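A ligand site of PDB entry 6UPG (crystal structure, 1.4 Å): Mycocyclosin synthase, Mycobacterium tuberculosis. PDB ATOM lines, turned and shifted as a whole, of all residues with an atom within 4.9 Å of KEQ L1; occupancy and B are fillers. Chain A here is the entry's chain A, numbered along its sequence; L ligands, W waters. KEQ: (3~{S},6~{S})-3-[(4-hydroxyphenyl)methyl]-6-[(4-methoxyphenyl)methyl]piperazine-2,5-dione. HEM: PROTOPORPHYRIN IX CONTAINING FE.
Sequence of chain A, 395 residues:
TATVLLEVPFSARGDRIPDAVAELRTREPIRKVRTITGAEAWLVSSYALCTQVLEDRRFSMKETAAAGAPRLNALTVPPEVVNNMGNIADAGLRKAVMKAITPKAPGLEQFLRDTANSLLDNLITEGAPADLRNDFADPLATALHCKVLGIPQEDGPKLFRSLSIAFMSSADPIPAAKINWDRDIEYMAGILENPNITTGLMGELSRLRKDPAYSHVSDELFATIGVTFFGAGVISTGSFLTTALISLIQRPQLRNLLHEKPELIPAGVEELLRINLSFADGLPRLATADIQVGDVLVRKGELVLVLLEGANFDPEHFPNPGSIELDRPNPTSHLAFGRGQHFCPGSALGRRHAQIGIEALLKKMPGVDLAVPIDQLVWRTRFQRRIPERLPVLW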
ATOM      1  N   MET A  61       6.819 -15.745  -6.921  1.00  0.00           N
ATOM      2  CA  MET A  61       7.205 -14.447  -7.459  1.00  0.00           C
ATOM      3  C   MET A  61       8.429 -14.586  -8.368  1.00  0.00           C
ATOM      4  O   MET A  61       8.461 -14.055  -9.485  1.00  0.00           O
ATOM      5  CB  MET A  61       7.477 -13.452  -6.327  1.00  0.00           C
ATOM      6  CG  MET A  61       8.212 -12.176  -6.773  1.00  0.00           C
ATOM      7  SD  MET A  61       8.636 -11.140  -5.335  1.00  0.00           S
ATOM      8  CE  MET A  61       7.001 -10.666  -4.829  1.00  0.00           C
ATOM      9  N   THR A  76      11.158  -4.155 -15.718  1.00  0.00           N
ATOM     10  CA  THR A  76      11.911  -2.908 -15.708  1.00  0.00           C
ATOM     11  C   THR A  76      13.192  -3.027 -14.904  1.00  0.00           C
ATOM     12  O   THR A  76      13.924  -2.044 -14.752  1.00  0.00           O
ATOM     13  CB  THR A  76      11.071  -1.750 -15.170  1.00  0.00           C
ATOM     14  OG1 THR A  76      10.815  -1.945 -13.778  1.00  0.00           O
ATOM     15  CG2 THR A  76       9.733  -1.661 -15.921  1.00  0.00           C
ATOM     16  N   VAL A  77      13.481  -4.222 -14.391  1.00  0.00           N
ATOM     17  CA  VAL A  77      14.701  -4.530 -13.643  1.00  0.00           C
ATOM     18  C   VAL A  77      15.286  -5.807 -14.219  1.00  0.00           C
ATOM     19  O   VAL A  77      14.579  -6.567 -14.900  1.00  0.00           O
ATOM     20  CB  VAL A  77      14.399  -4.705 -12.130  1.00  0.00           C
ATOM     21  CG1 VAL A  77      13.854  -3.409 -11.542  1.00  0.00           C
ATOM     22  CG2 VAL A  77      13.422  -5.851 -11.893  1.00  0.00           C
ATOM     23  N   VAL A  81      16.541  -9.539 -10.125  1.00  0.00           N
ATOM     24  CA  VAL A  81      16.028  -8.609  -9.138  1.00  0.00           C
ATOM     25  C   VAL A  81      14.564  -8.890  -8.797  1.00  0.00           C
ATOM     26  O   VAL A  81      14.059  -8.434  -7.774  1.00  0.00           O
ATOM     27  CB  VAL A  81      16.308  -7.161  -9.607  1.00  0.00           C
ATOM     28  CG1 VAL A  81      15.787  -6.131  -8.621  1.00  0.00           C
ATOM     29  CG2 VAL A  81      17.813  -6.957  -9.823  1.00  0.00           C
ATOM     30  N   VAL A  82      13.869  -9.655  -9.633  1.00  0.00           N
ATOM     31  CA  VAL A  82      12.528 -10.077  -9.243  1.00  0.00           C
ATOM     32  C   VAL A  82      12.570 -10.913  -7.972  1.00  0.00           C
ATOM     33  O   VAL A  82      11.635 -10.896  -7.160  1.00  0.00           O
ATOM     34  CB  VAL A  82      11.821 -10.788 -10.414  1.00  0.00           C
ATOM     35  CG1 VAL A  82      10.460 -11.321 -10.007  1.00  0.00           C
ATOM     36  CG2 VAL A  82      11.673  -9.821 -11.574  1.00  0.00           C
ATOM     37  N   ASN A  84      14.535 -10.225  -5.462  1.00  0.00           N
ATOM     38  CA  ASN A  84      15.385  -9.350  -4.649  1.00  0.00           C
ATOM     39  C   ASN A  84      15.432  -9.776  -3.182  1.00  0.00           C
ATOM     40  O   ASN A  84      16.517  -9.946  -2.613  1.00  0.00           O
ATOM     41  CB  ASN A  84      14.867  -7.908  -4.773  1.00  0.00           C
ATOM     42  CG  ASN A  84      15.820  -6.884  -4.187  1.00  0.00           C
ATOM     43  OD1 ASN A  84      17.033  -6.992  -4.338  1.00  0.00           O
ATOM     44  ND2 ASN A  84      15.259  -5.862  -3.540  1.00  0.00           N
ATOM     45  N   ALA A 166      10.537   3.765 -13.849  1.00  0.00           N
ATOM     46  CA  ALA A 166      10.909   2.482 -13.249  1.00  0.00           C
ATOM     47  C   ALA A 166       9.688   1.684 -12.846  1.00  0.00           C
ATOM     48  O   ALA A 166       9.703   0.448 -12.889  1.00  0.00           O
ATOM     49  CB  ALA A 166      11.775   2.738 -12.021  1.00  0.00           C
ATOM     50  N   PHE A 167       8.626   2.365 -12.408  1.00  0.00           N
ATOM     51  CA  PHE A 167       7.405   1.709 -11.977  1.00  0.00           C
ATOM     52  C   PHE A 167       6.304   1.730 -13.040  1.00  0.00           C
ATOM     53  O   PHE A 167       5.136   1.493 -12.718  1.00  0.00           O
ATOM     54  CB  PHE A 167       6.973   2.199 -10.602  1.00  0.00           C
ATOM     55  CG  PHE A 167       7.837   1.628  -9.512  1.00  0.00           C
ATOM     56  CD1 PHE A 167       7.557   0.372  -9.005  1.00  0.00           C
ATOM     57  CD2 PHE A 167       8.976   2.294  -9.090  1.00  0.00           C
ATOM     58  CE1 PHE A 167       8.361  -0.192  -8.036  1.00  0.00           C
ATOM     59  CE2 PHE A 167       9.811   1.714  -8.106  1.00  0.00           C
ATOM     60  CZ  PHE A 167       9.490   0.475  -7.592  1.00  0.00           C
ATOM     61  N   TRP A 181      18.271   2.733 -14.457  1.00  0.00           N
ATOM     62  CA  TRP A 181      18.703   1.653 -13.567  1.00  0.00           C
ATOM     63  C   TRP A 181      20.225   1.588 -13.486  1.00  0.00           C
ATOM     64  O   TRP A 181      20.800   1.575 -12.388  1.00  0.00           O
ATOM     65  CB  TRP A 181      18.146   0.315 -14.044  1.00  0.00           C
ATOM     66  CG  TRP A 181      18.628  -0.870 -13.223  1.00  0.00           C
ATOM     67  CD1 TRP A 181      19.675  -1.694 -13.503  1.00  0.00           C
ATOM     68  CD2 TRP A 181      18.087  -1.313 -11.974  1.00  0.00           C
ATOM     69  NE1 TRP A 181      19.812  -2.630 -12.515  1.00  0.00           N
ATOM     70  CE2 TRP A 181      18.856  -2.416 -11.560  1.00  0.00           C
ATOM     71  CE3 TRP A 181      17.021  -0.890 -11.174  1.00  0.00           C
ATOM     72  CZ2 TRP A 181      18.578  -3.112 -10.380  1.00  0.00           C
ATOM     73  CZ3 TRP A 181      16.757  -1.573 -10.007  1.00  0.00           C
ATOM     74  CH2 TRP A 181      17.544  -2.671  -9.607  1.00  0.00           C
ATOM     75  N   VAL A 227      19.211   0.725  -4.542  1.00  0.00           N
ATOM     76  CA  VAL A 227      18.306   1.215  -5.592  1.00  0.00           C
ATOM     77  C   VAL A 227      16.892   0.715  -5.358  1.00  0.00           C
ATOM     78  O   VAL A 227      15.920   1.466  -5.470  1.00  0.00           O
ATOM     79  CB  VAL A 227      18.812   0.818  -6.993  1.00  0.00           C
ATOM     80  CG1 VAL A 227      17.779   1.239  -8.046  1.00  0.00           C
ATOM     81  CG2 VAL A 227      20.145   1.470  -7.294  1.00  0.00           C
ATOM     82  N   THR A 228      16.753  -0.577  -5.033  1.00  0.00           N
ATOM     83  CA  THR A 228      15.430  -1.179  -4.918  1.00  0.00           C
ATOM     84  C   THR A 228      14.693  -0.701  -3.686  1.00  0.00           C
ATOM     85  O   THR A 228      13.470  -0.506  -3.727  1.00  0.00           O
ATOM     86  CB  THR A 228      15.510  -2.709  -4.929  1.00  0.00           C
ATOM     87  OG1 THR A 228      16.376  -3.154  -3.872  1.00  0.00           O
ATOM     88  CG2 THR A 228      16.014  -3.238  -6.257  1.00  0.00           C
ATOM     89  N   GLY A 231      13.553   2.823  -4.361  1.00  0.00           N
ATOM     90  CA  GLY A 231      12.489   2.929  -5.342  1.00  0.00           C
ATOM     91  C   GLY A 231      11.175   2.367  -4.832  1.00  0.00           C
ATOM     92  O   GLY A 231      10.136   3.039  -4.888  1.00  0.00           O
ATOM     93  N   ALA A 232      11.196   1.141  -4.315  1.00  0.00           N
ATOM     94  CA  ALA A 232       9.974   0.537  -3.803  1.00  0.00           C
ATOM     95  C   ALA A 232       9.422   1.327  -2.633  1.00  0.00           C
ATOM     96  O   ALA A 232       8.206   1.561  -2.544  1.00  0.00           O
ATOM     97  CB  ALA A 232      10.231  -0.921  -3.392  1.00  0.00           C
ATOM     98  N   SER A 236       5.987   3.569  -3.027  1.00  0.00           N
ATOM     99  CA  SER A 236       4.873   2.971  -2.302  1.00  0.00           C
ATOM    100  C   SER A 236       4.355   3.911  -1.234  1.00  0.00           C
ATOM    101  O   SER A 236       3.134   4.111  -1.123  1.00  0.00           O
ATOM    102  CB  SER A 236       5.316   1.641  -1.696  1.00  0.00           C
ATOM    103  OG  SER A 236       5.677   0.734  -2.733  1.00  0.00           O
ATOM    104  N   PHE A 279      -2.133   0.129  -5.531  1.00  0.00           N
ATOM    105  CA  PHE A 279      -1.595  -0.886  -6.439  1.00  0.00           C
ATOM    106  C   PHE A 279      -2.479  -0.998  -7.666  1.00  0.00           C
ATOM    107  O   PHE A 279      -3.652  -1.362  -7.576  1.00  0.00           O
ATOM    108  CB  PHE A 279      -1.410  -2.238  -5.739  1.00  0.00           C
ATOM    109  CG  PHE A 279      -0.092  -2.377  -5.034  1.00  0.00           C
ATOM    110  CD1 PHE A 279       0.201  -1.597  -3.933  1.00  0.00           C
ATOM    111  CD2 PHE A 279       0.886  -3.258  -5.493  1.00  0.00           C
ATOM    112  CE1 PHE A 279       1.430  -1.710  -3.282  1.00  0.00           C
ATOM    113  CE2 PHE A 279       2.113  -3.358  -4.852  1.00  0.00           C
ATOM    114  CZ  PHE A 279       2.386  -2.584  -3.746  1.00  0.00           C
ATOM    115  N   GLN A 384       2.505   1.084 -12.240  1.00  0.00           N
ATOM    116  CA  GLN A 384       2.294   0.059 -11.221  1.00  0.00           C
ATOM    117  C   GLN A 384       1.560   0.607 -10.000  1.00  0.00           C
ATOM    118  O   GLN A 384       1.150  -0.168  -9.129  1.00  0.00           O
ATOM    119  CB  GLN A 384       3.627  -0.565 -10.797  1.00  0.00           C
ATOM    120  CG  GLN A 384       4.270  -1.408 -11.892  1.00  0.00           C
ATOM    121  CD  GLN A 384       5.654  -1.916 -11.510  1.00  0.00           C
ATOM    122  OE1 GLN A 384       5.873  -2.342 -10.374  1.00  0.00           O
ATOM    123  NE2 GLN A 384       6.592  -1.845 -12.446  1.00  0.00           N
ATOM    124  N   ARG A 385       1.372   1.919  -9.944  1.00  0.00           N
ATOM    125  CA  ARG A 385       0.563   2.551  -8.913  1.00  0.00           C
ATOM    126  C   ARG A 385      -0.499   3.404  -9.580  1.00  0.00           C
ATOM    127  O   ARG A 385      -0.350   3.841 -10.730  1.00  0.00           O
ATOM    128  CB  ARG A 385       1.404   3.424  -7.965  1.00  0.00           C
ATOM    129  CG  ARG A 385       2.459   2.661  -7.145  1.00  0.00           C
ATOM    130  CD  ARG A 385       1.846   1.677  -6.127  1.00  0.00           C
ATOM    131  NE  ARG A 385       2.915   1.003  -5.383  1.00  0.00           N
ATOM    132  CZ  ARG A 385       3.572  -0.062  -5.825  1.00  0.00           C
ATOM    133  NH1 ARG A 385       4.554  -0.595  -5.096  1.00  0.00           N
ATOM    134  NH2 ARG A 385       3.253  -0.600  -6.996  1.00  0.00           N
HETATM  135  CA  KEQ L   1      11.951  -5.912  -5.339  1.00  0.00           C
HETATM  136  CB  KEQ L   1      11.005  -6.736  -7.940  1.00  0.00           C
HETATM  137  NB  KEQ L   1      11.287  -7.177  -5.510  1.00  0.00           N
HETATM  138  OB  KEQ L   1      10.720  -7.112  -9.039  1.00  0.00           O
HETATM  139  CD1 KEQ L   1      12.547  -1.749  -6.999  1.00  0.00           C
HETATM  140  CD2 KEQ L   1      11.004  -2.671  -8.580  1.00  0.00           C
HETATM  141  CD3 KEQ L   1       8.347  -6.280  -4.747  1.00  0.00           C
HETATM  142  CE1 KEQ L   1      12.974  -0.828  -7.948  1.00  0.00           C
HETATM  143  CE2 KEQ L   1      11.423  -1.757  -9.527  1.00  0.00           C
HETATM  144  CE3 KEQ L   1       7.676  -5.014  -4.234  1.00  0.00           C
HETATM  145  CAA KEQ L   1      12.067  -4.920  -6.491  1.00  0.00           C
HETATM  146  CAB KEQ L   1      10.659  -7.626  -6.743  1.00  0.00           C
HETATM  147  CAY KEQ L   1       6.299  -2.934  -3.287  1.00  0.00           C
HETATM  148  CBA KEQ L   1      11.151  -3.701  -6.245  1.00  0.00           C
HETATM  149  CBB KEQ L   1       9.138  -7.758  -6.565  1.00  0.00           C
HETATM  150  CD4 KEQ L   1       7.950  -5.444  -7.027  1.00  0.00           C
HETATM  151  CE4 KEQ L   1       7.376  -4.349  -6.583  1.00  0.00           C
HETATM  152  CGA KEQ L   1      11.570  -2.678  -7.306  1.00  0.00           C
HETATM  153  CGB KEQ L   1       8.476  -6.485  -6.045  1.00  0.00           C
HETATM  154  CZA KEQ L   1      12.420  -0.837  -9.224  1.00  0.00           C
HETATM  155  CZB KEQ L   1       7.228  -4.123  -5.098  1.00  0.00           C
HETATM  156  NA  KEQ L   1      11.695  -5.487  -7.774  1.00  0.00           N
HETATM  157  OA  KEQ L   1      12.435  -5.636  -4.289  1.00  0.00           O
HETATM  158  OAX KEQ L   1      12.875   0.082 -10.178  1.00  0.00           O
HETATM  159  OAY KEQ L   1       6.607  -2.948  -4.665  1.00  0.00           O
HETATM  160  CHA HEM L   2       6.596  -5.826  -0.747  1.00  0.00           C
HETATM  161  CHB HEM L   2       3.041  -2.592  -0.266  1.00  0.00           C
HETATM  162  CHC HEM L   2       6.205   0.460   1.756  1.00  0.00           C
HETATM  163  CHD HEM L   2       9.849  -2.385   0.282  1.00  0.00           C
HETATM  164  C1A HEM L   2       5.340  -5.258  -0.727  1.00  0.00           C
HETATM  165  C2A HEM L   2       4.104  -5.909  -1.099  1.00  0.00           C
HETATM  166  C3A HEM L   2       3.121  -5.009  -0.956  1.00  0.00           C
HETATM  167  C4A HEM L   2       3.700  -3.765  -0.513  1.00  0.00           C
HETATM  168  CMA HEM L   2       1.615  -5.213  -1.250  1.00  0.00           C
HETATM  169  CAA HEM L   2       3.971  -7.396  -1.537  1.00  0.00           C
HETATM  170  CBA HEM L   2       4.351  -7.572  -2.998  1.00  0.00           C
HETATM  171  CGA HEM L   2       4.083  -8.986  -3.451  1.00  0.00           C
HETATM  172  O1A HEM L   2       4.172  -9.235  -4.679  1.00  0.00           O
HETATM  173  O2A HEM L   2       3.782  -9.862  -2.610  1.00  0.00           O
HETATM  174  C1B HEM L   2       3.587  -1.483   0.349  1.00  0.00           C
HETATM  175  C2B HEM L   2       2.842  -0.320   0.786  1.00  0.00           C
HETATM  176  C3B HEM L   2       3.726   0.544   1.338  1.00  0.00           C
HETATM  177  C4B HEM L   2       5.035  -0.078   1.278  1.00  0.00           C
HETATM  178  CMB HEM L   2       1.321  -0.145   0.601  1.00  0.00           C
HETATM  179  CAB HEM L   2       3.488   1.920   1.985  1.00  0.00           C
HETATM  180  CBB HEM L   2       2.327   2.306   2.510  1.00  0.00           C
HETATM  181  C1C HEM L   2       7.474  -0.058   1.570  1.00  0.00           C
HETATM  182  C2C HEM L   2       8.706   0.519   2.056  1.00  0.00           C
HETATM  183  C3C HEM L   2       9.715  -0.264   1.640  1.00  0.00           C
HETATM  184  C4C HEM L   2       9.142  -1.362   0.887  1.00  0.00           C
HETATM  185  CMC HEM L   2       8.783   1.816   2.896  1.00  0.00           C
HETATM  186  CAC HEM L   2      11.237  -0.127   1.861  1.00  0.00           C
HETATM  187  CBC HEM L   2      11.851   0.933   2.402  1.00  0.00           C
HETATM  188  C1D HEM L   2       9.292  -3.559  -0.147  1.00  0.00           C
HETATM  189  C2D HEM L   2      10.005  -4.722  -0.670  1.00  0.00           C
HETATM  190  C3D HEM L   2       9.105  -5.670  -0.951  1.00  0.00           C
HETATM  191  C4D HEM L   2       7.792  -5.145  -0.623  1.00  0.00           C
HETATM  192  CMD HEM L   2      11.531  -4.810  -0.854  1.00  0.00           C
HETATM  193  CAD HEM L   2       9.401  -7.089  -1.508  1.00  0.00           C
HETATM  194  CBD HEM L   2       9.397  -8.082  -0.337  1.00  0.00           C
HETATM  195  CGD HEM L   2       9.565  -9.524  -0.765  1.00  0.00           C
HETATM  196  O1D HEM L   2       9.543  -9.815  -1.990  1.00  0.00           O
HETATM  197  O2D HEM L   2       9.710 -10.386   0.128  1.00  0.00           O
HETATM  198  NA  HEM L   2       5.061  -3.952  -0.366  1.00  0.00           N
HETATM  199  NB  HEM L   2       4.912  -1.302   0.650  1.00  0.00           N
HETATM  200  NC  HEM L   2       7.769  -1.219   0.877  1.00  0.00           N
HETATM  201  ND  HEM L   2       7.941  -3.850  -0.144  1.00  0.00           N
HETATM  202 FE   HEM L   2       6.412  -2.657   0.481  1.00  0.00          FE
HETATM  203  O   HOH W   1       4.633  -2.830  -7.982  1.00  0.00           O
HETATM  204  O   HOH W   2       8.049  -8.298 -10.163  1.00  0.00           O
HETATM  205  O   HOH W   3       9.880  -5.197 -10.901  1.00  0.00           O
HETATM  206  O   HOH W   4      13.543   0.092 -12.976  1.00  0.00           O
HETATM  207  O   HOH W   5       7.737  -4.259 -10.035  1.00  0.00           O
HETATM  208  O   HOH W   6      14.483   2.007  -9.505  1.00  0.00           O
HETATM  209  O   HOH W   7      11.588  -9.383  -3.707  1.00  0.00           O
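OA of KEQ L1 is in hydrogen-bond range of ND2 of Asn 84 (2.9 Å). An oxygen (OAY) of KEQ L1 sits at hydrogen-bond distance from the guanidinium group (NH1) of Arg 385 (3.2 Å).
The backbone carbonyl oxygen of Ala 166 is in hydrogen-bond range of the side-chain hydroxyl of Thr 76 (2.8 Å). The backbone carbonyl oxygen of Ala 232 sits at hydrogen-bond distance from the side-chain hydroxyl of Ser 236 (2.7 Å). O of Phe 167 lies within hydrogen-bond range of N of Gln 384 (2.7 Å). The guanidinium group (NH1) of Arg 385 sits at hydrogen-bond distance from the side-chain hydroxyl (OG) of Ser 236 (2.9 Å). ND2 of Asn 84 lies within hydrogen-bond range of OG1 of Thr 228 (2.9 Å).
Merely in contact with KEQ L1: Ala 166, Val 82, Val 81, Phe 167, Val 77, Thr 228, Met 61, Ser 236 and Phe 279. Hydrophobic or aromatic side chains that line KEQ L1: Met 61, Val 77, Val 82, Ala 166, Phe 167 and Phe 279.
Water W7 bridges an oxygen (O1D) of HEM L2 (2.7 Å) and a nitrogen (NB) of KEQ L1 (2.9 Å). Water W4 bridges the backbone carbonyl oxygen of Thr 76 and an oxygen (OAX) of KEQ L1. Water W1 lies within hydrogen-bond range of OE1 of Gln 384 (2.7 Å) and NH2 of Arg 385 (2.8 Å).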
